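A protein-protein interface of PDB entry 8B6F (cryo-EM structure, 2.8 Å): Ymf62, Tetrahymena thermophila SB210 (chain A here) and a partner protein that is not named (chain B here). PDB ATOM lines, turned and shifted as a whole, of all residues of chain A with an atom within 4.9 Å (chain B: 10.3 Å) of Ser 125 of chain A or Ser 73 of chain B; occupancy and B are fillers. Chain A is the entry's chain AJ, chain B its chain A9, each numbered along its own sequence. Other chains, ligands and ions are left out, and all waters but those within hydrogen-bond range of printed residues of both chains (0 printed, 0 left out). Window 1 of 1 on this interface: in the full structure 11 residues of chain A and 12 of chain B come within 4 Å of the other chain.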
ATOM      1  N   LEU A 120     -33.339  25.977 -12.685  1.00  0.00           N
ATOM      2  CA  LEU A 120     -33.664  24.574 -12.905  1.00  0.00           C
ATOM      3  C   LEU A 120     -32.774  23.914 -13.949  1.00  0.00           C
ATOM      4  O   LEU A 120     -32.344  22.773 -13.750  1.00  0.00           O
ATOM      5  CB  LEU A 120     -35.133  24.431 -13.315  1.00  0.00           C
ATOM      6  CG  LEU A 120     -36.190  24.665 -12.229  1.00  0.00           C
ATOM      7  CD1 LEU A 120     -37.581  24.446 -12.798  1.00  0.00           C
ATOM      8  CD2 LEU A 120     -35.974  23.781 -11.010  1.00  0.00           C
ATOM      9  N   TYR A 121     -32.495  24.584 -15.057  1.00  0.00           N
ATOM     10  CA  TYR A 121     -31.794  23.921 -16.151  1.00  0.00           C
ATOM     11  C   TYR A 121     -30.554  24.658 -16.628  1.00  0.00           C
ATOM     12  O   TYR A 121     -29.556  24.014 -16.956  1.00  0.00           O
ATOM     13  CB  TYR A 121     -32.754  23.730 -17.338  1.00  0.00           C
ATOM     14  CG  TYR A 121     -32.092  23.132 -18.559  1.00  0.00           C
ATOM     15  CD1 TYR A 121     -32.033  21.758 -18.736  1.00  0.00           C
ATOM     16  CD2 TYR A 121     -31.527  23.943 -19.535  1.00  0.00           C
ATOM     17  CE1 TYR A 121     -31.428  21.207 -19.846  1.00  0.00           C
ATOM     18  CE2 TYR A 121     -30.920  23.401 -20.649  1.00  0.00           C
ATOM     19  CZ  TYR A 121     -30.874  22.034 -20.799  1.00  0.00           C
ATOM     20  OH  TYR A 121     -30.271  21.490 -21.906  1.00  0.00           O
ATOM     21  N   TYR A 122     -30.583  25.988 -16.671  1.00  0.00           N
ATOM     22  CA  TYR A 122     -29.595  26.711 -17.462  1.00  0.00           C
ATOM     23  C   TYR A 122     -28.300  26.989 -16.710  1.00  0.00           C
ATOM     24  O   TYR A 122     -27.216  26.848 -17.287  1.00  0.00           O
ATOM     25  CB  TYR A 122     -30.199  28.017 -17.976  1.00  0.00           C
ATOM     26  CG  TYR A 122     -31.177  27.785 -19.100  1.00  0.00           C
ATOM     27  CD1 TYR A 122     -30.737  27.637 -20.407  1.00  0.00           C
ATOM     28  CD2 TYR A 122     -32.537  27.686 -18.852  1.00  0.00           C
ATOM     29  CE1 TYR A 122     -31.626  27.411 -21.437  1.00  0.00           C
ATOM     30  CE2 TYR A 122     -33.433  27.461 -19.874  1.00  0.00           C
ATOM     31  CZ  TYR A 122     -32.971  27.326 -21.164  1.00  0.00           C
ATOM     32  OH  TYR A 122     -33.868  27.102 -22.181  1.00  0.00           O
ATOM     33  N   THR A 123     -28.372  27.399 -15.447  1.00  0.00           N
ATOM     34  CA  THR A 123     -27.140  27.656 -14.708  1.00  0.00           C
ATOM     35  C   THR A 123     -26.282  26.405 -14.586  1.00  0.00           C
ATOM     36  O   THR A 123     -25.085  26.469 -14.915  1.00  0.00           O
ATOM     37  CB  THR A 123     -27.465  28.244 -13.331  1.00  0.00           C
ATOM     38  OG1 THR A 123     -28.374  29.342 -13.478  1.00  0.00           O
ATOM     39  CG2 THR A 123     -26.198  28.737 -12.654  1.00  0.00           C
ATOM     40  N   PRO A 124     -26.803  25.254 -14.149  1.00  0.00           N
ATOM     41  CA  PRO A 124     -25.928  24.078 -14.021  1.00  0.00           C
ATOM     42  C   PRO A 124     -25.437  23.551 -15.356  1.00  0.00           C
ATOM     43  O   PRO A 124     -24.274  23.145 -15.466  1.00  0.00           O
ATOM     44  CB  PRO A 124     -26.813  23.051 -13.297  1.00  0.00           C
ATOM     45  CG  PRO A 124     -28.012  23.800 -12.828  1.00  0.00           C
ATOM     46  CD  PRO A 124     -28.188  24.936 -13.768  1.00  0.00           C
ATOM     47  N   SER A 125     -26.293  23.549 -16.377  1.00  0.00           N
ATOM     48  CA  SER A 125     -25.868  23.091 -17.695  1.00  0.00           C
ATOM     49  C   SER A 125     -24.761  23.976 -18.250  1.00  0.00           C
ATOM     50  O   SER A 125     -23.789  23.476 -18.828  1.00  0.00           O
ATOM     51  CB  SER A 125     -27.060  23.055 -18.651  1.00  0.00           C
ATOM     52  OG  SER A 125     -27.596  24.350 -18.847  1.00  0.00           O
ATOM     53  N   LEU A 126     -24.891  25.293 -18.090  1.00  0.00           N
ATOM     54  CA  LEU A 126     -23.826  26.190 -18.521  1.00  0.00           C
ATOM     55  C   LEU A 126     -22.546  25.944 -17.735  1.00  0.00           C
ATOM     56  O   LEU A 126     -21.446  25.990 -18.298  1.00  0.00           O
ATOM     57  CB  LEU A 126     -24.260  27.647 -18.372  1.00  0.00           C
ATOM     58  CG  LEU A 126     -23.147  28.662 -18.655  1.00  0.00           C
ATOM     59  CD1 LEU A 126     -22.608  28.503 -20.064  1.00  0.00           C
ATOM     60  CD2 LEU A 126     -23.650  30.058 -18.458  1.00  0.00           C
ATOM     61  N   VAL A 127     -22.663  25.685 -16.433  1.00  0.00           N
ATOM     62  CA  VAL A 127     -21.474  25.419 -15.629  1.00  0.00           C
ATOM     63  C   VAL A 127     -20.749  24.190 -16.159  1.00  0.00           C
ATOM     64  O   VAL A 127     -19.526  24.198 -16.339  1.00  0.00           O
ATOM     65  CB  VAL A 127     -21.853  25.265 -14.144  1.00  0.00           C
ATOM     66  CG1 VAL A 127     -20.728  24.608 -13.360  1.00  0.00           C
ATOM     67  CG2 VAL A 127     -22.191  26.620 -13.541  1.00  0.00           C
ATOM     68  N   LEU A 128     -21.492  23.113 -16.418  1.00  0.00           N
ATOM     69  CA  LEU A 128     -20.866  21.902 -16.937  1.00  0.00           C
ATOM     70  C   LEU A 128     -20.232  22.152 -18.298  1.00  0.00           C
ATOM     71  O   LEU A 128     -19.110  21.707 -18.561  1.00  0.00           O
ATOM     72  CB  LEU A 128     -21.891  20.772 -17.028  1.00  0.00           C
ATOM     73  CG  LEU A 128     -22.421  20.217 -15.707  1.00  0.00           C
ATOM     74  CD1 LEU A 128     -23.490  19.177 -15.974  1.00  0.00           C
ATOM     75  CD2 LEU A 128     -21.301  19.625 -14.866  1.00  0.00           C
ATOM     76  N   PHE A 129     -20.941  22.856 -19.183  1.00  0.00           N
ATOM     77  CA  PHE A 129     -20.404  23.112 -20.513  1.00  0.00           C
ATOM     78  C   PHE A 129     -19.126  23.937 -20.440  1.00  0.00           C
ATOM     79  O   PHE A 129     -18.146  23.636 -21.129  1.00  0.00           O
ATOM     80  CB  PHE A 129     -21.449  23.822 -21.371  1.00  0.00           C
ATOM     81  CG  PHE A 129     -20.992  24.095 -22.772  1.00  0.00           C
ATOM     82  CD1 PHE A 129     -21.035  23.100 -23.733  1.00  0.00           C
ATOM     83  CD2 PHE A 129     -20.520  25.347 -23.128  1.00  0.00           C
ATOM     84  CE1 PHE A 129     -20.615  23.346 -25.024  1.00  0.00           C
ATOM     85  CE2 PHE A 129     -20.098  25.601 -24.418  1.00  0.00           C
ATOM     86  CZ  PHE A 129     -20.146  24.598 -25.368  1.00  0.00           C
ATOM     87  N   ALA B  65     -21.266  11.046  -8.402  1.00  0.00           N
ATOM     88  CA  ALA B  65     -21.794  12.362  -8.058  1.00  0.00           C
ATOM     89  C   ALA B  65     -21.854  13.269  -9.279  1.00  0.00           C
ATOM     90  O   ALA B  65     -22.830  14.003  -9.469  1.00  0.00           O
ATOM     91  CB  ALA B  65     -20.940  13.000  -6.964  1.00  0.00           C
ATOM     92  N   LEU B  66     -20.821  13.231 -10.121  1.00  0.00           N
ATOM     93  CA  LEU B  66     -20.836  14.031 -11.340  1.00  0.00           C
ATOM     94  C   LEU B  66     -21.962  13.596 -12.267  1.00  0.00           C
ATOM     95  O   LEU B  66     -22.637  14.435 -12.872  1.00  0.00           O
ATOM     96  CB  LEU B  66     -19.485  13.929 -12.047  1.00  0.00           C
ATOM     97  CG  LEU B  66     -19.352  14.686 -13.369  1.00  0.00           C
ATOM     98  CD1 LEU B  66     -19.622  16.170 -13.185  1.00  0.00           C
ATOM     99  CD2 LEU B  66     -17.975  14.464 -13.961  1.00  0.00           C
ATOM    100  N   LEU B  67     -22.175  12.287 -12.398  1.00  0.00           N
ATOM    101  CA  LEU B  67     -23.275  11.796 -13.221  1.00  0.00           C
ATOM    102  C   LEU B  67     -24.618  12.254 -12.670  1.00  0.00           C
ATOM    103  O   LEU B  67     -25.506  12.652 -13.431  1.00  0.00           O
ATOM    104  CB  LEU B  67     -23.228  10.271 -13.310  1.00  0.00           C
ATOM    105  CG  LEU B  67     -22.708   9.693 -14.625  1.00  0.00           C
ATOM    106  CD1 LEU B  67     -21.342  10.254 -14.961  1.00  0.00           C
ATOM    107  CD2 LEU B  67     -22.662   8.179 -14.559  1.00  0.00           C
ATOM    108  N   GLY B  68     -24.791  12.192 -11.349  1.00  0.00           N
ATOM    109  CA  GLY B  68     -26.038  12.647 -10.758  1.00  0.00           C
ATOM    110  C   GLY B  68     -26.268  14.132 -10.957  1.00  0.00           C
ATOM    111  O   GLY B  68     -27.387  14.565 -11.237  1.00  0.00           O
ATOM    112  N   VAL B  69     -25.212  14.933 -10.811  1.00  0.00           N
ATOM    113  CA  VAL B  69     -25.338  16.372 -11.023  1.00  0.00           C
ATOM    114  C   VAL B  69     -25.688  16.663 -12.475  1.00  0.00           C
ATOM    115  O   VAL B  69     -26.510  17.540 -12.767  1.00  0.00           O
ATOM    116  CB  VAL B  69     -24.044  17.088 -10.591  1.00  0.00           C
ATOM    117  CG1 VAL B  69     -24.038  18.537 -11.060  1.00  0.00           C
ATOM    118  CG2 VAL B  69     -23.888  17.024  -9.081  1.00  0.00           C
ATOM    119  N   ALA B  70     -25.073  15.936 -13.410  1.00  0.00           N
ATOM    120  CA  ALA B  70     -25.404  16.119 -14.819  1.00  0.00           C
ATOM    121  C   ALA B  70     -26.854  15.746 -15.095  1.00  0.00           C
ATOM    122  O   ALA B  70     -27.551  16.446 -15.837  1.00  0.00           O
ATOM    123  CB  ALA B  70     -24.465  15.287 -15.690  1.00  0.00           C
ATOM    124  N   TYR B  71     -27.325  14.643 -14.513  1.00  0.00           N
ATOM    125  CA  TYR B  71     -28.722  14.266 -14.694  1.00  0.00           C
ATOM    126  C   TYR B  71     -29.650  15.335 -14.135  1.00  0.00           C
ATOM    127  O   TYR B  71     -30.666  15.672 -14.752  1.00  0.00           O
ATOM    128  CB  TYR B  71     -28.993  12.917 -14.027  1.00  0.00           C
ATOM    129  CG  TYR B  71     -30.448  12.519 -14.059  1.00  0.00           C
ATOM    130  CD1 TYR B  71     -31.017  11.986 -15.206  1.00  0.00           C
ATOM    131  CD2 TYR B  71     -31.252  12.677 -12.940  1.00  0.00           C
ATOM    132  CE1 TYR B  71     -32.348  11.624 -15.239  1.00  0.00           C
ATOM    133  CE2 TYR B  71     -32.584  12.319 -12.961  1.00  0.00           C
ATOM    134  CZ  TYR B  71     -33.126  11.792 -14.115  1.00  0.00           C
ATOM    135  OH  TYR B  71     -34.452  11.434 -14.141  1.00  0.00           O
ATOM    136  N   ALA B  72     -29.324  15.873 -12.959  1.00  0.00           N
ATOM    137  CA  ALA B  72     -30.139  16.937 -12.384  1.00  0.00           C
ATOM    138  C   ALA B  72     -30.138  18.171 -13.274  1.00  0.00           C
ATOM    139  O   ALA B  72     -31.185  18.792 -13.493  1.00  0.00           O
ATOM    140  CB  ALA B  72     -29.628  17.292 -10.989  1.00  0.00           C
ATOM    141  N   SER B  73     -28.970  18.541 -13.799  1.00  0.00           N
ATOM    142  CA  SER B  73     -28.883  19.714 -14.658  1.00  0.00           C
ATOM    143  C   SER B  73     -29.717  19.538 -15.917  1.00  0.00           C
ATOM    144  O   SER B  73     -30.399  20.470 -16.357  1.00  0.00           O
ATOM    145  CB  SER B  73     -27.425  19.979 -15.026  1.00  0.00           C
ATOM    146  OG  SER B  73     -26.599  19.979 -13.875  1.00  0.00           O
ATOM    147  N   GLY B  74     -29.677  18.351 -16.511  1.00  0.00           N
ATOM    148  CA  GLY B  74     -30.338  18.117 -17.776  1.00  0.00           C
ATOM    149  C   GLY B  74     -31.824  17.847 -17.676  1.00  0.00           C
ATOM    150  O   GLY B  74     -32.629  18.562 -18.279  1.00  0.00           O
ATOM    151  N   PHE B  75     -32.201  16.823 -16.919  1.00  0.00           N
ATOM    152  CA  PHE B  75     -33.557  16.290 -16.965  1.00  0.00           C
ATOM    153  C   PHE B  75     -34.287  16.349 -15.634  1.00  0.00           C
ATOM    154  O   PHE B  75     -35.470  16.697 -15.605  1.00  0.00           O
ATOM    155  CB  PHE B  75     -33.516  14.834 -17.454  1.00  0.00           C
ATOM    156  CG  PHE B  75     -32.601  14.618 -18.626  1.00  0.00           C
ATOM    157  CD1 PHE B  75     -31.244  14.420 -18.431  1.00  0.00           C
ATOM    158  CD2 PHE B  75     -33.095  14.613 -19.920  1.00  0.00           C
ATOM    159  CE1 PHE B  75     -30.397  14.223 -19.501  1.00  0.00           C
ATOM    160  CE2 PHE B  75     -32.251  14.417 -20.997  1.00  0.00           C
ATOM    161  CZ  PHE B  75     -30.900  14.221 -20.787  1.00  0.00           C
ATOM    162  N   GLY B  76     -33.626  16.007 -14.533  1.00  0.00           N
ATOM    163  CA  GLY B  76     -34.318  15.849 -13.270  1.00  0.00           C
ATOM    164  C   GLY B  76     -34.978  17.111 -12.756  1.00  0.00           C
ATOM    165  O   GLY B  76     -36.182  17.122 -12.490  1.00  0.00           O
ATOM    166  N   LEU B  77     -34.202  18.185 -12.612  1.00  0.00           N
ATOM    167  CA  LEU B  77     -34.751  19.425 -12.074  1.00  0.00           C
ATOM    168  C   LEU B  77     -35.808  20.018 -12.997  1.00  0.00           C
ATOM    169  O   LEU B  77     -36.847  20.501 -12.532  1.00  0.00           O
ATOM    170  CB  LEU B  77     -33.626  20.431 -11.830  1.00  0.00           C
ATOM    171  CG  LEU B  77     -32.614  20.042 -10.751  1.00  0.00           C
ATOM    172  CD1 LEU B  77     -31.469  21.036 -10.715  1.00  0.00           C
ATOM    173  CD2 LEU B  77     -33.274  19.945  -9.385  1.00  0.00           C
ATOM    174  N   ILE B  78     -35.567  19.988 -14.307  1.00  0.00           N
ATOM    175  CA  ILE B  78     -36.515  20.581 -15.243  1.00  0.00           C
ATOM    176  C   ILE B  78     -37.827  19.807 -15.244  1.00  0.00           C
ATOM    177  O   ILE B  78     -38.908  20.393 -15.375  1.00  0.00           O
ATOM    178  CB  ILE B  78     -35.895  20.666 -16.652  1.00  0.00           C
ATOM    179  CG1 ILE B  78     -36.805  21.449 -17.604  1.00  0.00           C
ATOM    180  CG2 ILE B  78     -35.620  19.281 -17.214  1.00  0.00           C
ATOM    181  CD1 ILE B  78     -36.972  22.914 -17.238  1.00  0.00           C
ATOM    182  N   SER B  79     -37.762  18.482 -15.099  1.00  0.00           N
ATOM    183  CA  SER B  79     -38.988  17.694 -15.044  1.00  0.00           C
ATOM    184  C   SER B  79     -39.733  17.922 -13.735  1.00  0.00           C
ATOM    185  O   SER B  79     -40.964  18.036 -13.728  1.00  0.00           O
ATOM    186  CB  SER B  79     -38.666  16.211 -15.229  1.00  0.00           C
ATOM    187  OG  SER B  79     -37.834  15.735 -14.184  1.00  0.00           O
ATOM    188  N   LYS B  80     -39.012  17.989 -12.620  1.00  0.00           N
ATOM    189  CA  LYS B  80     -39.655  18.197 -11.330  1.00  0.00           C
ATOM    190  C   LYS B  80     -40.196  19.618 -11.227  1.00  0.00           C
ATOM    191  O   LYS B  80     -39.533  20.583 -11.613  1.00  0.00           O
ATOM    192  CB  LYS B  80     -38.672  17.926 -10.192  1.00  0.00           C
ATOM    193  CG  LYS B  80     -39.039  16.726  -9.323  1.00  0.00           C
ATOM    194  CD  LYS B  80     -39.055  15.421 -10.110  1.00  0.00           C
ATOM    195  CE  LYS B  80     -37.652  14.963 -10.479  1.00  0.00           C
ATOM    196  NZ  LYS B  80     -37.673  13.782 -11.389  1.00  0.00           N
ATOM    197  N   MET B 105     -28.301  26.375  -6.000  1.00  0.00           N
ATOM    198  CA  MET B 105     -27.777  25.233  -6.738  1.00  0.00           C
ATOM    199  C   MET B 105     -27.315  24.141  -5.786  1.00  0.00           C
ATOM    200  O   MET B 105     -27.556  22.952  -6.027  1.00  0.00           O
ATOM    201  CB  MET B 105     -26.624  25.667  -7.642  1.00  0.00           C
ATOM    202  CG  MET B 105     -27.022  26.575  -8.798  1.00  0.00           C
ATOM    203  SD  MET B 105     -28.269  25.874  -9.887  1.00  0.00           S
ATOM    204  CE  MET B 105     -29.747  26.527  -9.114  1.00  0.00           C
ATOM    205  N   GLN B 106     -26.650  24.523  -4.696  1.00  0.00           N
ATOM    206  CA  GLN B 106     -26.222  23.536  -3.712  1.00  0.00           C
ATOM    207  C   GLN B 106     -27.422  22.783  -3.152  1.00  0.00           C
ATOM    208  O   GLN B 106     -27.409  21.550  -3.058  1.00  0.00           O
ATOM    209  CB  GLN B 106     -25.433  24.229  -2.599  1.00  0.00           C
ATOM    210  CG  GLN B 106     -24.857  23.291  -1.546  1.00  0.00           C
ATOM    211  CD  GLN B 106     -25.843  22.950  -0.446  1.00  0.00           C
ATOM    212  OE1 GLN B 106     -26.862  23.617  -0.279  1.00  0.00           O
ATOM    213  NE2 GLN B 106     -25.541  21.902   0.312  1.00  0.00           N
ATOM    214  N   LEU B 108     -30.414  22.363  -4.472  1.00  0.00           N
ATOM    215  CA  LEU B 108     -31.117  21.562  -5.469  1.00  0.00           C
ATOM    216  C   LEU B 108     -30.318  20.329  -5.869  1.00  0.00           C
ATOM    217  O   LEU B 108     -30.896  19.265  -6.116  1.00  0.00           O
ATOM    218  CB  LEU B 108     -31.429  22.413  -6.700  1.00  0.00           C
ATOM    219  CG  LEU B 108     -32.561  23.432  -6.555  1.00  0.00           C
ATOM    220  CD1 LEU B 108     -32.636  24.311  -7.788  1.00  0.00           C
ATOM    221  CD2 LEU B 108     -33.897  22.743  -6.311  1.00  0.00           C
ATOM    222  N   LEU B 109     -28.996  20.451  -5.953  1.00  0.00           N
ATOM    223  CA  LEU B 109     -28.156  19.357  -6.414  1.00  0.00           C
ATOM    224  C   LEU B 109     -27.651  18.466  -5.289  1.00  0.00           C
ATOM    225  O   LEU B 109     -27.025  17.438  -5.572  1.00  0.00           O
ATOM    226  CB  LEU B 109     -26.958  19.909  -7.194  1.00  0.00           C
ATOM    227  CG  LEU B 109     -27.294  20.796  -8.396  1.00  0.00           C
ATOM    228  CD1 LEU B 109     -26.027  21.364  -9.004  1.00  0.00           C
ATOM    229  CD2 LEU B 109     -28.080  20.021  -9.438  1.00  0.00           C
ATOM    230  N   THR B 110     -27.892  18.824  -4.028  1.00  0.00           N
ATOM    231  CA  THR B 110     -27.458  17.962  -2.931  1.00  0.00           C
ATOM    232  C   THR B 110     -28.062  16.570  -3.020  1.00  0.00           C
ATOM    233  O   THR B 110     -27.309  15.586  -2.909  1.00  0.00           O
ATOM    234  CB  THR B 110     -27.786  18.629  -1.589  1.00  0.00           C
ATOM    235  OG1 THR B 110     -26.956  19.784  -1.410  1.00  0.00           O
ATOM    236  CG2 THR B 110     -27.560  17.663  -0.424  1.00  0.00           C
ATOM    237  N   TYR B 112     -29.233  14.775  -5.629  1.00  0.00           N
ATOM    238  CA  TYR B 112     -28.684  14.038  -6.763  1.00  0.00           C
ATOM    239  C   TYR B 112     -27.205  13.738  -6.567  1.00  0.00           C
ATOM    240  O   TYR B 112     -26.746  12.629  -6.860  1.00  0.00           O
ATOM    241  CB  TYR B 112     -28.906  14.827  -8.052  1.00  0.00           C
ATOM    242  CG  TYR B 112     -30.365  15.025  -8.392  1.00  0.00           C
ATOM    243  CD1 TYR B 112     -31.063  16.130  -7.922  1.00  0.00           C
ATOM    244  CD2 TYR B 112     -31.040  14.115  -9.193  1.00  0.00           C
ATOM    245  CE1 TYR B 112     -32.392  16.317  -8.232  1.00  0.00           C
ATOM    246  CE2 TYR B 112     -32.371  14.294  -9.508  1.00  0.00           C
ATOM    247  CZ  TYR B 112     -33.041  15.398  -9.026  1.00  0.00           C
ATOM    248  OH  TYR B 112     -34.367  15.583  -9.338  1.00  0.00           O
ATOM    249  N   ALA B 113     -26.437  14.718  -6.091  1.00  0.00           N
ATOM    250  CA  ALA B 113     -25.011  14.493  -5.884  1.00  0.00           C
ATOM    251  C   ALA B 113     -24.767  13.408  -4.842  1.00  0.00           C
ATOM    252  O   ALA B 113     -23.920  12.529  -5.037  1.00  0.00           O
ATOM    253  CB  ALA B 113     -24.329  15.795  -5.469  1.00  0.00           C
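The backbone carbonyl oxygen (O) of Val 69 of chain B sits at hydrogen-bond distance from the side-chain hydroxyl (OG) of Ser 73 of chain B, at 2.7 Å.
The backbone carbonyl oxygen (O) of Ala 72 of chain B lies within hydrogen-bond range of the backbone NH (N) of Leu 77 of chain B (3.2 Å).
O of Tyr 121 of chain A sits at hydrogen-bond distance from OG of Ser 125 of chain A (2.7 Å).
OG of Ser 125 of chain A is in hydrogen-bond range of O of Tyr 122 of chain A, 3.0 Å away.
Ser 73 of chain B touches Leu 120 of chain A (O to O, 3.99 Å).
O of Leu 120 of chain A touches CB of Leu 77 of chain B, at 3.3 Å.
CD1 of Tyr 121 of chain A touches O of Ser 73 of chain B, at 3.2 Å.
Gly 74 of chain B touches Tyr 121 of chain A.
Ser 73 of chain B touches Pro 124 of chain A (OG to CB, 3.1 Å).
Pro 124 of chain A touches Met 105 of chain B (CG to SD, 3.6 Å).
Ser 73 of chain B touches Ser 125 of chain A (CB to N, 3.98 Å).
Leu 128 of chain A touches Ala 70 of chain B (CD1 to CA, 3.8 Å).
Ser 73 of chain B touches Leu 128 of chain A.
Printed residues of chain A within 4 Å of Ser 73 of chain B: Leu 120 (3.99 Å), Tyr 121 (3.2 Å), Pro 124 (3.1 Å), Ser 125 (3.98 Å) and Leu 128 (3.8 Å).
Of chain B, only Ser 73 (3.2 Å) and Gly 74 (3.3 Å) come within 4 Å of Tyr 121 of chain A.
Pro 124 of chain A touches two residues of chain B.
Leu 128 of chain A touches just these residues of chain B: Ala 70 (3.8 Å) and Ser 73 (3.8 Å).
Of the printed residues of chain A, Gly 74 of chain B touches Tyr 121 (3.3 Å).
Of the printed residues of chain A, Ala 70 of chain B touches Leu 128 (3.8 Å).
Of the printed residues of chain A, Met 105 of chain B touches Pro 124 (3.6 Å).
Printed residues of chain A within 4 Å of Leu 77 of chain B: Leu 120 (3.3 Å).
Of the printed residues of chain B, Leu 120 of chain A touches Ser 73 (3.99 Å) and Leu 77 (3.3 Å).
Tyr 71 of chain B touches none of the printed residues of chain A.
The nearest printed residue of chain B that does not touch Ser 125 of chain A is Gly 74 of chain B (5.8 Å).
The nearest printed residue of chain A that does not touch Ser 73 of chain B is Tyr 122 of chain A (5.5 Å).
Hydrophobic or aromatic side chains of chain B within 4 Å of the printed part of chain A: Leu 77 and Met 105.
Hydrophobic or aromatic side chains of chain A that line the printed part of chain B: Leu 120, Tyr 121, Pro 124 and Leu 128.
Among the printed residues, 9 pairs touch across the chains.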
